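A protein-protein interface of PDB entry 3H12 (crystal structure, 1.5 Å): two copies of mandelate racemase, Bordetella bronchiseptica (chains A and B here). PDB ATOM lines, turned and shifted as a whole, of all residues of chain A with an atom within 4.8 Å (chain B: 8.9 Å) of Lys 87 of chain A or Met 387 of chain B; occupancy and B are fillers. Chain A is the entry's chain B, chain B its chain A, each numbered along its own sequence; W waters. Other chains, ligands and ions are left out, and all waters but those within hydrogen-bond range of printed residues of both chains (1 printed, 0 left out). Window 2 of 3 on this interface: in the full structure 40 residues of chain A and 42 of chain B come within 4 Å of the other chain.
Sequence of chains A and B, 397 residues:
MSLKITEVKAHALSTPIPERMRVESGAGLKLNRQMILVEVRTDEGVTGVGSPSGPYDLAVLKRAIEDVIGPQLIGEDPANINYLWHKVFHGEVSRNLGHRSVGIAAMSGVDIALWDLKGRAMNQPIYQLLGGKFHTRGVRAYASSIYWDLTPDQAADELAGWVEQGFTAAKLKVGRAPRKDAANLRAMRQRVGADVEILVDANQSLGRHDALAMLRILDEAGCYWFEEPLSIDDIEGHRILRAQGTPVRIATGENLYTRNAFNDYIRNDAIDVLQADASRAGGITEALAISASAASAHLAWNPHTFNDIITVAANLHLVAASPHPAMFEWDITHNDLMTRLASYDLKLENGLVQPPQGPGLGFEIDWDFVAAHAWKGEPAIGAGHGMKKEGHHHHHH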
ATOM      1  N   GLN A  72      25.304 -10.405  -4.641  1.00  0.00           N
ATOM      2  CA  GLN A  72      25.328  -9.869  -3.264  1.00  0.00           C
ATOM      3  C   GLN A  72      25.845 -10.854  -2.257  1.00  0.00           C
ATOM      4  O   GLN A  72      26.149 -10.512  -1.135  1.00  0.00           O
ATOM      5  CB  GLN A  72      23.897  -9.443  -2.833  1.00  0.00           C
ATOM      6  CG  GLN A  72      23.243  -8.367  -3.707  1.00  0.00           C
ATOM      7  CD  GLN A  72      24.016  -7.049  -3.661  1.00  0.00           C
ATOM      8  OE1 GLN A  72      24.156  -6.429  -4.731  1.00  0.00           O
ATOM      9  NE2 GLN A  72      24.527  -6.587  -2.439  1.00  0.00           N
ATOM     10  N   GLU A  76      30.780 -13.789   0.600  1.00  0.00           N
ATOM     11  CA  GLU A  76      30.309 -13.620   1.949  1.00  0.00           C
ATOM     12  C   GLU A  76      30.342 -14.931   2.728  1.00  0.00           C
ATOM     13  O   GLU A  76      30.229 -16.026   2.118  1.00  0.00           O
ATOM     14  CB  GLU A  76      28.843 -13.168   1.937  1.00  0.00           C
ATOM     15  CG  GLU A  76      28.672 -11.778   1.384  1.00  0.00           C
ATOM     16  CD  GLU A  76      28.899 -10.672   2.461  1.00  0.00           C
ATOM     17  OE1 GLU A  76      29.065 -11.029   3.696  1.00  0.00           O
ATOM     18  OE2 GLU A  76      28.789  -9.466   2.127  1.00  0.00           O
ATOM     19  N   TYR A  83      21.880 -11.566   8.321  1.00  0.00           N
ATOM     20  CA  TYR A  83      22.427 -10.406   7.591  1.00  0.00           C
ATOM     21  C   TYR A  83      22.162 -10.490   6.057  1.00  0.00           C
ATOM     22  O   TYR A  83      21.769  -9.479   5.435  1.00  0.00           O
ATOM     23  CB  TYR A  83      23.950 -10.412   7.854  1.00  0.00           C
ATOM     24  CG  TYR A  83      24.697  -9.462   6.965  1.00  0.00           C
ATOM     25  CD1 TYR A  83      24.561  -8.052   7.114  1.00  0.00           C
ATOM     26  CD2 TYR A  83      25.555  -9.974   5.958  1.00  0.00           C
ATOM     27  CE1 TYR A  83      25.286  -7.188   6.297  1.00  0.00           C
ATOM     28  CE2 TYR A  83      26.307  -9.085   5.130  1.00  0.00           C
ATOM     29  CZ  TYR A  83      26.084  -7.708   5.281  1.00  0.00           C
ATOM     30  OH  TYR A  83      26.760  -6.777   4.478  1.00  0.00           O
ATOM     31  N   LEU A  84      22.375 -11.696   5.491  1.00  0.00           N
ATOM     32  CA  LEU A  84      22.339 -11.787   4.011  1.00  0.00           C
ATOM     33  C   LEU A  84      20.892 -11.572   3.540  1.00  0.00           C
ATOM     34  O   LEU A  84      20.669 -11.004   2.447  1.00  0.00           O
ATOM     35  CB  LEU A  84      22.889 -13.153   3.579  1.00  0.00           C
ATOM     36  CG  LEU A  84      24.414 -13.279   3.814  1.00  0.00           C
ATOM     37  CD1 LEU A  84      24.795 -14.703   3.467  1.00  0.00           C
ATOM     38  CD2 LEU A  84      25.166 -12.288   2.946  1.00  0.00           C
ATOM     39  N   TRP A  85      19.914 -12.011   4.326  1.00  0.00           N
ATOM     40  CA  TRP A  85      18.551 -11.792   3.888  1.00  0.00           C
ATOM     41  C   TRP A  85      18.260 -10.287   3.728  1.00  0.00           C
ATOM     42  O   TRP A  85      17.754  -9.818   2.720  1.00  0.00           O
ATOM     43  CB  TRP A  85      17.574 -12.369   4.976  1.00  0.00           C
ATOM     44  CG  TRP A  85      16.121 -12.465   4.434  1.00  0.00           C
ATOM     45  CD1 TRP A  85      15.534 -13.630   3.883  1.00  0.00           C
ATOM     46  CD2 TRP A  85      15.147 -11.443   4.361  1.00  0.00           C
ATOM     47  NE1 TRP A  85      14.236 -13.339   3.492  1.00  0.00           N
ATOM     48  CE2 TRP A  85      13.997 -12.014   3.743  1.00  0.00           C
ATOM     49  CE3 TRP A  85      15.118 -10.084   4.707  1.00  0.00           C
ATOM     50  CZ2 TRP A  85      12.834 -11.276   3.470  1.00  0.00           C
ATOM     51  CZ3 TRP A  85      13.928  -9.337   4.463  1.00  0.00           C
ATOM     52  CH2 TRP A  85      12.809  -9.949   3.857  1.00  0.00           C
ATOM     53  N   HIS A  86      18.623  -9.517   4.789  1.00  0.00           N
ATOM     54  CA  HIS A  86      18.414  -8.048   4.720  1.00  0.00           C
ATOM     55  C   HIS A  86      19.308  -7.356   3.768  1.00  0.00           C
ATOM     56  O   HIS A  86      18.854  -6.425   3.061  1.00  0.00           O
ATOM     57  CB  HIS A  86      18.500  -7.520   6.201  1.00  0.00           C
ATOM     58  CG  HIS A  86      17.379  -8.038   7.041  1.00  0.00           C
ATOM     59  ND1 HIS A  86      16.149  -7.392   7.128  1.00  0.00           N
ATOM     60  CD2 HIS A  86      17.239  -9.209   7.706  1.00  0.00           C
ATOM     61  CE1 HIS A  86      15.345  -8.123   7.893  1.00  0.00           C
ATOM     62  NE2 HIS A  86      15.951  -9.245   8.203  1.00  0.00           N
ATOM     63  N   LYS A  87      20.551  -7.819   3.607  1.00  0.00           N
ATOM     64  CA  LYS A  87      21.410  -7.211   2.592  1.00  0.00           C
ATOM     65  C   LYS A  87      20.787  -7.304   1.217  1.00  0.00           C
ATOM     66  O   LYS A  87      20.787  -6.328   0.458  1.00  0.00           O
ATOM     67  CB  LYS A  87      22.748  -7.957   2.575  1.00  0.00           C
ATOM     68  CG  LYS A  87      23.845  -7.355   1.657  1.00  0.00           C
ATOM     69  CD  LYS A  87      25.065  -8.293   1.430  1.00  0.00           C
ATOM     70  CE  LYS A  87      26.082  -7.436   0.669  1.00  0.00           C
ATOM     71  NZ  LYS A  87      27.109  -8.210   0.073  1.00  0.00           N
ATOM     72  N   VAL A  88      20.191  -8.482   0.887  1.00  0.00           N
ATOM     73  CA  VAL A  88      19.653  -8.690  -0.460  1.00  0.00           C
ATOM     74  C   VAL A  88      18.285  -7.940  -0.564  1.00  0.00           C
ATOM     75  O   VAL A  88      18.056  -7.329  -1.605  1.00  0.00           O
ATOM     76  CB  VAL A  88      19.427 -10.220  -0.626  1.00  0.00           C
ATOM     77  CG1 VAL A  88      18.501 -10.576  -1.797  1.00  0.00           C
ATOM     78  CG2 VAL A  88      20.817 -10.925  -0.882  1.00  0.00           C
ATOM     79  N   PHE A  89      17.447  -7.908   0.523  1.00  0.00           N
ATOM     80  CA  PHE A  89      16.147  -7.303   0.388  1.00  0.00           C
ATOM     81  C   PHE A  89      16.346  -5.806   0.165  1.00  0.00           C
ATOM     82  O   PHE A  89      15.674  -5.191  -0.722  1.00  0.00           O
ATOM     83  CB  PHE A  89      15.301  -7.592   1.647  1.00  0.00           C
ATOM     84  CG  PHE A  89      13.982  -6.909   1.638  1.00  0.00           C
ATOM     85  CD1 PHE A  89      12.876  -7.577   1.096  1.00  0.00           C
ATOM     86  CD2 PHE A  89      13.821  -5.690   2.297  1.00  0.00           C
ATOM     87  CE1 PHE A  89      11.609  -6.977   1.115  1.00  0.00           C
ATOM     88  CE2 PHE A  89      12.538  -5.065   2.292  1.00  0.00           C
ATOM     89  CZ  PHE A  89      11.417  -5.754   1.720  1.00  0.00           C
ATOM     90  N   HIS A  90      17.161  -5.189   1.019  1.00  0.00           N
ATOM     91  CA  HIS A  90      17.328  -3.722   0.947  1.00  0.00           C
ATOM     92  C   HIS A  90      18.221  -3.296  -0.154  1.00  0.00           C
ATOM     93  O   HIS A  90      18.036  -2.200  -0.757  1.00  0.00           O
ATOM     94  CB  HIS A  90      17.875  -3.164   2.245  1.00  0.00           C
ATOM     95  CG  HIS A  90      16.913  -3.322   3.380  1.00  0.00           C
ATOM     96  ND1 HIS A  90      15.748  -2.560   3.478  1.00  0.00           N
ATOM     97  CD2 HIS A  90      16.918  -4.128   4.458  1.00  0.00           C
ATOM     98  CE1 HIS A  90      15.106  -2.865   4.602  1.00  0.00           C
ATOM     99  NE2 HIS A  90      15.772  -3.829   5.204  1.00  0.00           N
ATOM    100  N   GLY A  91      19.221  -4.124  -0.424  1.00  0.00           N
ATOM    101  CA  GLY A  91      20.203  -3.775  -1.499  1.00  0.00           C
ATOM    102  C   GLY A  91      19.608  -3.787  -2.887  1.00  0.00           C
ATOM    103  O   GLY A  91      19.963  -2.922  -3.718  1.00  0.00           O
ATOM    104  N   GLU A  92      18.784  -4.812  -3.194  1.00  0.00           N
ATOM    105  CA  GLU A  92      18.270  -4.989  -4.511  1.00  0.00           C
ATOM    106  C   GLU A  92      16.809  -5.333  -4.621  1.00  0.00           C
ATOM    107  O   GLU A  92      16.087  -4.770  -5.448  1.00  0.00           O
ATOM    108  CB  GLU A  92      19.041  -6.219  -5.106  1.00  0.00           C
ATOM    109  CG  GLU A  92      20.404  -5.858  -5.593  1.00  0.00           C
ATOM    110  CD  GLU A  92      20.342  -5.288  -6.985  1.00  0.00           C
ATOM    111  OE1 GLU A  92      19.268  -4.915  -7.508  1.00  0.00           O
ATOM    112  OE2 GLU A  92      21.379  -5.226  -7.634  1.00  0.00           O
ATOM    113  N   GLY B  26      18.529   7.468  -1.230  1.00  0.00           N
ATOM    114  CA  GLY B  26      18.353   6.161  -0.473  1.00  0.00           C
ATOM    115  C   GLY B  26      18.146   5.005  -1.395  1.00  0.00           C
ATOM    116  O   GLY B  26      18.242   3.900  -0.921  1.00  0.00           O
ATOM    117  N   ASN B 203      13.238   8.353   0.275  1.00  0.00           N
ATOM    118  CA  ASN B 203      13.451   7.024  -0.352  1.00  0.00           C
ATOM    119  C   ASN B 203      13.465   5.893   0.706  1.00  0.00           C
ATOM    120  O   ASN B 203      14.259   4.930   0.664  1.00  0.00           O
ATOM    121  CB  ASN B 203      14.847   6.945  -1.144  1.00  0.00           C
ATOM    122  CG  ASN B 203      14.760   7.698  -2.453  1.00  0.00           C
ATOM    123  OD1 ASN B 203      15.188   8.845  -2.519  1.00  0.00           O
ATOM    124  ND2 ASN B 203      14.177   7.058  -3.486  1.00  0.00           N
ATOM    125  N   GLN B 204      12.446   5.941   1.545  1.00  0.00           N
ATOM    126  CA  GLN B 204      12.184   4.874   2.603  1.00  0.00           C
ATOM    127  C   GLN B 204      13.313   4.738   3.594  1.00  0.00           C
ATOM    128  O   GLN B 204      13.475   3.650   4.153  1.00  0.00           O
ATOM    129  CB  GLN B 204      11.973   3.468   1.936  1.00  0.00           C
ATOM    130  CG  GLN B 204      10.942   3.510   0.759  1.00  0.00           C
ATOM    131  CD  GLN B 204      10.701   2.115   0.208  1.00  0.00           C
ATOM    132  OE1 GLN B 204      10.300   1.183   0.952  1.00  0.00           O
ATOM    133  NE2 GLN B 204      11.049   1.860  -1.074  1.00  0.00           N
ATOM    134  N   SER B 205      14.128   5.781   3.764  1.00  0.00           N
ATOM    135  CA  SER B 205      15.383   5.532   4.489  1.00  0.00           C
ATOM    136  C   SER B 205      15.244   5.821   6.009  1.00  0.00           C
ATOM    137  O   SER B 205      16.233   5.588   6.750  1.00  0.00           O
ATOM    138  CB  SER B 205      16.516   6.277   3.782  1.00  0.00           C
ATOM    139  OG  SER B 205      16.355   7.614   4.132  1.00  0.00           O
ATOM    140  N   ALA B 383      23.865  -0.647  -4.799  1.00  0.00           N
ATOM    141  CA  ALA B 383      22.974  -1.197  -3.733  1.00  0.00           C
ATOM    142  C   ALA B 383      22.223  -0.125  -3.037  1.00  0.00           C
ATOM    143  O   ALA B 383      22.794   0.946  -2.684  1.00  0.00           O
ATOM    144  CB  ALA B 383      23.751  -2.064  -2.718  1.00  0.00           C
ATOM    145  N   GLY B 384      20.923  -0.361  -2.846  1.00  0.00           N
ATOM    146  CA  GLY B 384      20.158   0.632  -2.179  1.00  0.00           C
ATOM    147  C   GLY B 384      20.383   0.634  -0.675  1.00  0.00           C
ATOM    148  O   GLY B 384      21.076  -0.226  -0.075  1.00  0.00           O
ATOM    149  N   HIS B 385      19.722   1.610  -0.034  1.00  0.00           N
ATOM    150  CA  HIS B 385      19.917   1.761   1.399  1.00  0.00           C
ATOM    151  C   HIS B 385      18.602   1.256   2.075  1.00  0.00           C
ATOM    152  O   HIS B 385      17.530   0.933   1.467  1.00  0.00           O
ATOM    153  CB  HIS B 385      20.232   3.198   1.756  1.00  0.00           C
ATOM    154  CG  HIS B 385      21.469   3.702   1.087  1.00  0.00           C
ATOM    155  ND1 HIS B 385      22.755   3.379   1.518  1.00  0.00           N
ATOM    156  CD2 HIS B 385      21.623   4.446  -0.039  1.00  0.00           C
ATOM    157  CE1 HIS B 385      23.636   3.964   0.712  1.00  0.00           C
ATOM    158  NE2 HIS B 385      22.962   4.678  -0.194  1.00  0.00           N
ATOM    159  N   GLY B 386      18.710   1.082   3.353  1.00  0.00           N
ATOM    160  CA  GLY B 386      17.596   0.552   4.121  1.00  0.00           C
ATOM    161  C   GLY B 386      18.151  -0.287   5.228  1.00  0.00           C
ATOM    162  O   GLY B 386      17.529  -0.358   6.293  1.00  0.00           O
ATOM    163  N   MET B 387      19.329  -0.878   4.999  1.00  0.00           N
ATOM    164  CA  MET B 387      19.995  -1.601   6.165  1.00  0.00           C
ATOM    165  C   MET B 387      20.212  -0.701   7.413  1.00  0.00           C
ATOM    166  O   MET B 387      20.156  -1.167   8.543  1.00  0.00           O
ATOM    167  CB  MET B 387      21.314  -2.271   5.750  1.00  0.00           C
ATOM    168  CG  MET B 387      21.152  -3.545   4.894  1.00  0.00           C
ATOM    169  SD  MET B 387      20.487  -4.752   6.015  1.00  0.00           S
ATOM    170  CE  MET B 387      22.003  -5.529   6.098  1.00  0.00           C
ATOM    171  N   LYS B 388      20.589   0.566   7.230  1.00  0.00           N
ATOM    172  CA  LYS B 388      20.768   1.464   8.411  1.00  0.00           C
ATOM    173  C   LYS B 388      19.524   1.584   9.301  1.00  0.00           C
ATOM    174  O   LYS B 388      19.546   1.281  10.546  1.00  0.00           O
ATOM    175  CB  LYS B 388      21.353   2.828   7.988  1.00  0.00           C
ATOM    176  CG  LYS B 388      21.726   3.703   9.221  1.00  0.00           C
ATOM    177  CD  LYS B 388      22.076   5.126   8.781  1.00  0.00           C
ATOM    178  CE  LYS B 388      22.003   6.149   9.918  1.00  0.00           C
ATOM    179  NZ  LYS B 388      22.404   7.442   9.255  1.00  0.00           N
ATOM    180  N   LYS B 389      18.403   1.977   8.725  1.00  0.00           N
ATOM    181  CA  LYS B 389      17.231   2.110   9.527  1.00  0.00           C
ATOM    182  C   LYS B 389      16.736   0.733   9.980  1.00  0.00           C
ATOM    183  O   LYS B 389      16.113   0.661  11.063  1.00  0.00           O
ATOM    184  CB  LYS B 389      16.116   2.938   8.877  1.00  0.00           C
ATOM    185  CG  LYS B 389      15.501   2.354   7.684  1.00  0.00           C
ATOM    186  CD  LYS B 389      14.246   1.696   8.137  1.00  0.00           C
ATOM    187  CE  LYS B 389      13.703   0.880   6.954  1.00  0.00           C
ATOM    188  NZ  LYS B 389      12.398   0.251   7.386  1.00  0.00           N
ATOM    189  N   GLU B 390      17.006  -0.318   9.152  1.00  0.00           N
ATOM    190  CA  GLU B 390      16.689  -1.681   9.624  1.00  0.00           C
ATOM    191  C   GLU B 390      17.398  -1.954  10.970  1.00  0.00           C
ATOM    192  O   GLU B 390      16.919  -2.735  11.797  1.00  0.00           O
ATOM    193  CB  GLU B 390      17.125  -2.776   8.636  1.00  0.00           C
ATOM    194  CG  GLU B 390      16.638  -4.184   9.001  1.00  0.00           C
ATOM    195  CD  GLU B 390      15.140  -4.317   8.773  1.00  0.00           C
ATOM    196  OE1 GLU B 390      14.675  -4.383   7.588  1.00  0.00           O
ATOM    197  OE2 GLU B 390      14.369  -4.238   9.766  1.00  0.00           O
ATOM    198  N   GLY B 391      18.610  -1.442  11.137  1.00  0.00           N
ATOM    199  CA  GLY B 391      19.284  -1.600  12.446  1.00  0.00           C
ATOM    200  C   GLY B 391      20.793  -1.920  12.260  1.00  0.00           C
ATOM    201  O   GLY B 391      21.449  -2.104  13.267  1.00  0.00           O
ATOM    202  N   HIS B 392      21.335  -1.914  11.036  1.00  0.00           N
ATOM    203  CA  HIS B 392      22.749  -2.301  10.842  1.00  0.00           C
ATOM    204  C   HIS B 392      23.555  -1.019  11.067  1.00  0.00           C
ATOM    205  O   HIS B 392      23.481  -0.101  10.247  1.00  0.00           O
ATOM    206  CB  HIS B 392      22.989  -2.952   9.444  1.00  0.00           C
ATOM    207  CG  HIS B 392      24.301  -3.665   9.346  1.00  0.00           C
ATOM    208  ND1 HIS B 392      24.476  -5.001   9.665  1.00  0.00           N
ATOM    209  CD2 HIS B 392      25.531  -3.205   8.992  1.00  0.00           C
ATOM    210  CE1 HIS B 392      25.753  -5.339   9.501  1.00  0.00           C
ATOM    211  NE2 HIS B 392      26.410  -4.258   9.117  1.00  0.00           N
ATOM    212  N   HIS B 393      24.377  -0.995  12.108  1.00  0.00           N
ATOM    213  CA  HIS B 393      25.090   0.250  12.587  1.00  0.00           C
ATOM    214  C   HIS B 393      26.033   0.941  11.569  1.00  0.00           C
ATOM    215  O   HIS B 393      26.873   0.204  10.980  1.00  0.00           O
ATOM    216  CB  HIS B 393      25.855  -0.158  13.897  1.00  0.00           C
ATOM    217  CG  HIS B 393      26.464   0.993  14.635  1.00  0.00           C
ATOM    218  ND1 HIS B 393      25.705   1.858  15.413  1.00  0.00           N
ATOM    219  CD2 HIS B 393      27.753   1.432  14.705  1.00  0.00           C
ATOM    220  CE1 HIS B 393      26.504   2.759  15.972  1.00  0.00           C
ATOM    221  NE2 HIS B 393      27.745   2.544  15.530  1.00  0.00           N
HETATM  222  O   HOH W   1      14.922  -0.571   1.909  1.00  0.00           O
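Of chain B, only Met 387 comes within 4 Å of Lys 87 of chain A. Of chain A, only Tyr 83, His 86, Lys 87 and His 90 come within 4 Å of Met 387 of chain B. Of the printed residues of chain A, Glu 390 of chain B touches His 86 and His 90. Of the printed residues of chain B, His 90 of chain A touches Gly 384, His 385, Gly 386, Met 387 and Glu 390. Printed residues of chain A within 4 Å of His 392 of chain B: Tyr 83 (3.7 Å). Of the printed residues of chain A, His 385 of chain B touches His 90. Of the printed residues of chain B, Tyr 83 of chain A touches Met 387 (3.7 Å) and His 392 (3.7 Å). Gln 204 of chain B touches none of the printed residues of chain A. The nearest residue of chain B that does not touch Lys 87 of chain A is Ala 383 of chain B (6.1 Å). The nearest printed residue of chain A that does not touch Met 387 of chain B is Gly 91 of chain A (5.7 Å).
Among the printed residues, merely in contact across the chains: Tyr 83 of chain A with Met 387 of chain B, Tyr 83 of chain A with His 392 of chain B, Lys 87 of chain A with Met 387 of chain B, His 90 of chain A with Gly 384 of chain B, His 90 of chain A with His 385 of chain B, His 90 of chain A with Gly 386 of chain B, His 90 of chain A with Met 387 of chain B and Gly 91 of chain A with Ala 383 of chain B.
The backbone carbonyl oxygen (O) of Met 387 of chain B sits at hydrogen-bond distance from the backbone NH (N) of His 392 of chain B (2.9 Å). The backbone carbonyl oxygen (O) of Gln 72 of chain A lies within hydrogen-bond range of the side-chain amino group (NZ) of Lys 87 of chain A (2.8 Å). NZ of Lys 87 of chain A lies within salt-bridge range of OE2 of Glu 76 of chain A, at 2.9 Å. The backbone NH of His 385 of chain B is in hydrogen-bond range of the backbone carbonyl oxygen of Gly 26 of chain B.
The side-chain carboxylate of Glu 390 of chain B sits at hydrogen-bond distance from a ring nitrogen (ND1) of His 86 of chain A, 3.4 Å away. The backbone carbonyl oxygen (O) of His 86 of chain A lies close to the side-chain sulfur (SD) of Met 387 of chain B (3.8 Å). N of Gly 384 of chain B is in hydrogen-bond range of O of Gly 91 of chain A (2.9 Å). A ring nitrogen (NE2) of His 90 of chain A sits at hydrogen-bond distance from the side-chain carboxylate (OE1) of Glu 390 of chain B, 2.7 Å away.
No position is printed for both chains.
Water W1 lies within hydrogen-bond range of a ring nitrogen (ND1) of His 90 of chain A (2.7 Å) and the backbone carbonyl oxygen of His 385 of chain B (3.0 Å).
Of the 15 printed residues of chain B, 7 touch a printed residue of chain A. Printed residues of chain B that touch a printed residue of chain A: Ala 383, Gly 384, His 385, Gly 386, Met 387, Glu 390 and His 392. Hydrophobic or aromatic side chains of chain B that line the printed part of chain A: Met 387 and His 392. Hydrophobic or aromatic side chains of chain A that line the printed part of chain B: Tyr 83, His 86 and His 90.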
